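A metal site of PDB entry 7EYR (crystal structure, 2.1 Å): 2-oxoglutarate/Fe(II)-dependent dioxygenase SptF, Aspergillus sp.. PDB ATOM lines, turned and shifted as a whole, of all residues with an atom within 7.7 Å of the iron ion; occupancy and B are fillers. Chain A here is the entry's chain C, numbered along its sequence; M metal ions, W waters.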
ATOM      1  N   LEU A 114      12.954 -20.902 -16.694  1.00  0.00           N
ATOM      2  CA  LEU A 114      12.503 -19.644 -17.291  1.00  0.00           C
ATOM      3  C   LEU A 114      13.660 -18.969 -18.016  1.00  0.00           C
ATOM      4  O   LEU A 114      14.231 -17.978 -17.559  1.00  0.00           O
ATOM      5  CB  LEU A 114      11.923 -18.721 -16.207  1.00  0.00           C
ATOM      6  CG  LEU A 114      10.867 -19.340 -15.290  1.00  0.00           C
ATOM      7  CD1 LEU A 114      10.752 -18.533 -14.001  1.00  0.00           C
ATOM      8  CD2 LEU A 114       9.517 -19.438 -15.992  1.00  0.00           C
ATOM      9  N   GLN A 123       5.814 -10.924 -23.067  1.00  0.00           N
ATOM     10  CA  GLN A 123       4.844 -11.957 -22.725  1.00  0.00           C
ATOM     11  C   GLN A 123       3.493 -11.327 -22.395  1.00  0.00           C
ATOM     12  O   GLN A 123       3.446 -10.228 -21.831  1.00  0.00           O
ATOM     13  CB  GLN A 123       5.348 -12.773 -21.522  1.00  0.00           C
ATOM     14  CG  GLN A 123       4.395 -13.860 -21.060  1.00  0.00           C
ATOM     15  CD  GLN A 123       4.972 -14.690 -19.921  1.00  0.00           C
ATOM     16  OE1 GLN A 123       5.522 -14.156 -18.959  1.00  0.00           O
ATOM     17  NE2 GLN A 123       4.841 -16.011 -20.036  1.00  0.00           N
ATOM     18  N   PRO A 124       2.390 -11.977 -22.767  1.00  0.00           N
ATOM     19  CA  PRO A 124       1.064 -11.474 -22.365  1.00  0.00           C
ATOM     20  C   PRO A 124       0.960 -11.369 -20.848  1.00  0.00           C
ATOM     21  O   PRO A 124       1.440 -12.220 -20.103  1.00  0.00           O
ATOM     22  CB  PRO A 124       0.101 -12.514 -22.926  1.00  0.00           C
ATOM     23  CG  PRO A 124       0.833 -13.130 -24.078  1.00  0.00           C
ATOM     24  CD  PRO A 124       2.285 -13.106 -23.702  1.00  0.00           C
ATOM     25  N   HIS A 126      -0.669 -11.541 -17.309  1.00  0.00           N
ATOM     26  CA  HIS A 126      -1.573 -12.610 -16.881  1.00  0.00           C
ATOM     27  C   HIS A 126      -1.472 -12.831 -15.377  1.00  0.00           C
ATOM     28  O   HIS A 126      -0.542 -12.381 -14.718  1.00  0.00           O
ATOM     29  CB  HIS A 126      -1.236 -13.917 -17.608  1.00  0.00           C
ATOM     30  CG  HIS A 126       0.146 -14.416 -17.332  1.00  0.00           C
ATOM     31  ND1 HIS A 126       1.256 -13.957 -18.018  1.00  0.00           N
ATOM     32  CD2 HIS A 126       0.604 -15.317 -16.434  1.00  0.00           C
ATOM     33  CE1 HIS A 126       2.332 -14.557 -17.549  1.00  0.00           C
ATOM     34  NE2 HIS A 126       1.966 -15.396 -16.590  1.00  0.00           N
ATOM     35  N   GLN A 127      -2.474 -13.537 -14.862  1.00  0.00           N
ATOM     36  CA  GLN A 127      -2.435 -14.113 -13.515  1.00  0.00           C
ATOM     37  C   GLN A 127      -2.181 -15.615 -13.640  1.00  0.00           C
ATOM     38  O   GLN A 127      -2.734 -16.274 -14.519  1.00  0.00           O
ATOM     39  CB  GLN A 127      -3.750 -13.863 -12.776  1.00  0.00           C
ATOM     40  CG  GLN A 127      -4.098 -12.393 -12.534  1.00  0.00           C
ATOM     41  CD  GLN A 127      -5.458 -12.220 -11.870  1.00  0.00           C
ATOM     42  OE1 GLN A 127      -6.483 -12.583 -12.435  1.00  0.00           O
ATOM     43  NE2 GLN A 127      -5.459 -11.671 -10.662  1.00  0.00           N
ATOM     44  N   ASP A 128      -1.330 -16.145 -12.758  1.00  0.00           N
ATOM     45  CA  ASP A 128      -0.956 -17.556 -12.884  1.00  0.00           C
ATOM     46  C   ASP A 128      -2.113 -18.498 -12.552  1.00  0.00           C
ATOM     47  O   ASP A 128      -2.127 -19.640 -13.031  1.00  0.00           O
ATOM     48  CB  ASP A 128       0.245 -17.860 -11.980  1.00  0.00           C
ATOM     49  CG  ASP A 128       1.554 -17.519 -12.635  1.00  0.00           C
ATOM     50  OD1 ASP A 128       1.539 -17.073 -13.799  1.00  0.00           O
ATOM     51  OD2 ASP A 128       2.605 -17.708 -11.986  1.00  0.00           O
ATOM     52  N   HIS A 129      -3.078 -18.063 -11.750  1.00  0.00           N
ATOM     53  CA  HIS A 129      -4.193 -18.930 -11.404  1.00  0.00           C
ATOM     54  C   HIS A 129      -5.291 -18.957 -12.475  1.00  0.00           C
ATOM     55  O   HIS A 129      -6.398 -19.415 -12.191  1.00  0.00           O
ATOM     56  CB  HIS A 129      -4.785 -18.543 -10.043  1.00  0.00           C
ATOM     57  CG  HIS A 129      -5.483 -17.214 -10.015  1.00  0.00           C
ATOM     58  ND1 HIS A 129      -5.546 -16.451  -8.880  1.00  0.00           N
ATOM     59  CD2 HIS A 129      -6.164 -16.534 -10.963  1.00  0.00           C
ATOM     60  CE1 HIS A 129      -6.233 -15.344  -9.127  1.00  0.00           C
ATOM     61  NE2 HIS A 129      -6.612 -15.374 -10.385  1.00  0.00           N
ATOM     62  N   ASN A 148       4.000 -18.682  -6.806  1.00  0.00           N
ATOM     63  CA  ASN A 148       5.221 -18.934  -7.559  1.00  0.00           C
ATOM     64  C   ASN A 148       6.390 -18.222  -6.882  1.00  0.00           C
ATOM     65  O   ASN A 148       6.240 -17.105  -6.392  1.00  0.00           O
ATOM     66  CB  ASN A 148       5.064 -18.445  -9.006  1.00  0.00           C
ATOM     67  CG  ASN A 148       6.328 -18.617  -9.845  1.00  0.00           C
ATOM     68  OD1 ASN A 148       7.339 -17.965  -9.587  1.00  0.00           O
ATOM     69  ND2 ASN A 148       6.264 -19.468 -10.859  1.00  0.00           N
ATOM     70  N   THR A 150      10.038 -17.131  -8.190  1.00  0.00           N
ATOM     71  CA  THR A 150      10.830 -17.001  -9.398  1.00  0.00           C
ATOM     72  C   THR A 150      12.228 -16.533  -9.009  1.00  0.00           C
ATOM     73  O   THR A 150      12.410 -15.389  -8.562  1.00  0.00           O
ATOM     74  CB  THR A 150      10.178 -16.041 -10.395  1.00  0.00           C
ATOM     75  OG1 THR A 150       9.046 -16.696 -10.995  1.00  0.00           O
ATOM     76  CG2 THR A 150      11.164 -15.665 -11.501  1.00  0.00           C
ATOM     77  N   THR A 163      11.001  -9.918 -15.239  1.00  0.00           N
ATOM     78  CA  THR A 163       9.560  -9.937 -14.975  1.00  0.00           C
ATOM     79  C   THR A 163       9.061  -8.565 -14.540  1.00  0.00           C
ATOM     80  O   THR A 163       9.724  -7.860 -13.780  1.00  0.00           O
ATOM     81  CB  THR A 163       9.232 -10.973 -13.903  1.00  0.00           C
ATOM     82  OG1 THR A 163       9.965 -12.185 -14.167  1.00  0.00           O
ATOM     83  CG2 THR A 163       7.742 -11.281 -13.889  1.00  0.00           C
ATOM     84  N   LEU A 197       5.459 -14.414  -6.297  1.00  0.00           N
ATOM     85  CA  LEU A 197       4.341 -14.237  -7.222  1.00  0.00           C
ATOM     86  C   LEU A 197       3.141 -15.074  -6.791  1.00  0.00           C
ATOM     87  O   LEU A 197       3.031 -16.249  -7.172  1.00  0.00           O
ATOM     88  CB  LEU A 197       4.761 -14.586  -8.653  1.00  0.00           C
ATOM     89  CG  LEU A 197       5.423 -13.478  -9.468  1.00  0.00           C
ATOM     90  CD1 LEU A 197       5.778 -13.978 -10.860  1.00  0.00           C
ATOM     91  CD2 LEU A 197       4.519 -12.259  -9.544  1.00  0.00           C
ATOM     92  N   MET A 201      -1.484 -12.114  -8.720  1.00  0.00           N
ATOM     93  CA  MET A 201      -0.716 -10.951  -9.153  1.00  0.00           C
ATOM     94  C   MET A 201      -0.604 -10.929 -10.674  1.00  0.00           C
ATOM     95  O   MET A 201      -0.168 -11.913 -11.287  1.00  0.00           O
ATOM     96  CB  MET A 201       0.672 -10.978  -8.500  1.00  0.00           C
ATOM     97  CG  MET A 201       1.637  -9.893  -8.983  1.00  0.00           C
ATOM     98  SD  MET A 201       0.907  -8.252  -9.242  1.00  0.00           S
ATOM     99  CE  MET A 201       0.371  -7.838  -7.585  1.00  0.00           C
ATOM    100  N   HIS A 203       1.131 -10.085 -14.037  1.00  0.00           N
ATOM    101  CA  HIS A 203       2.550 -10.017 -14.351  1.00  0.00           C
ATOM    102  C   HIS A 203       2.774 -10.565 -15.754  1.00  0.00           C
ATOM    103  O   HIS A 203       1.873 -11.136 -16.372  1.00  0.00           O
ATOM    104  CB  HIS A 203       3.390 -10.812 -13.351  1.00  0.00           C
ATOM    105  CG  HIS A 203       3.193 -12.284 -13.458  1.00  0.00           C
ATOM    106  ND1 HIS A 203       2.008 -12.906 -13.123  1.00  0.00           N
ATOM    107  CD2 HIS A 203       4.024 -13.273 -13.885  1.00  0.00           C
ATOM    108  CE1 HIS A 203       2.122 -14.210 -13.325  1.00  0.00           C
ATOM    109  NE2 HIS A 203       3.333 -14.452 -13.797  1.00  0.00           N
ATOM    110  N   SER A 204       4.012 -10.398 -16.229  1.00  0.00           N
ATOM    111  CA  SER A 204       4.471 -10.957 -17.496  1.00  0.00           C
ATOM    112  C   SER A 204       5.950 -10.682 -17.639  1.00  0.00           C
ATOM    113  O   SER A 204       6.467  -9.671 -17.139  1.00  0.00           O
ATOM    114  CB  SER A 204       3.711 -10.365 -18.687  1.00  0.00           C
ATOM    115  OG  SER A 204       4.450  -9.290 -19.255  1.00  0.00           O
ATOM    116  N   ALA A 205       6.634 -11.564 -18.361  1.00  0.00           N
ATOM    117  CA  ALA A 205       8.019 -11.325 -18.727  1.00  0.00           C
ATOM    118  C   ALA A 205       8.086 -10.317 -19.862  1.00  0.00           C
ATOM    119  O   ALA A 205       7.224 -10.275 -20.740  1.00  0.00           O
ATOM    120  CB  ALA A 205       8.701 -12.630 -19.146  1.00  0.00           C
HETATM  121 FE    FE M   1       3.408 -16.387 -14.971  1.00  0.00          FE
HETATM  122  O   HOH W   1       4.614 -17.196 -13.443  1.00  0.00           O
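Within 4 Å of the iron ion: His 126, Asp 128 and His 203.
Along chain A the residues within 4 Å of the iron ion span positions 126 to 203.
The iron ion is bound by water W1 (2.1 Å), NE2 of His 203 (2.3 Å), OD1 of Asp 128 (2.3 Å) and NE2 of His 126 (2.4 Å).
O of Met 201 is in hydrogen-bond range of ND1 of His 203, 3.0 Å away.
A ring nitrogen (ND1) of His 126 sits at hydrogen-bond distance from the backbone carbonyl oxygen of Pro 124.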
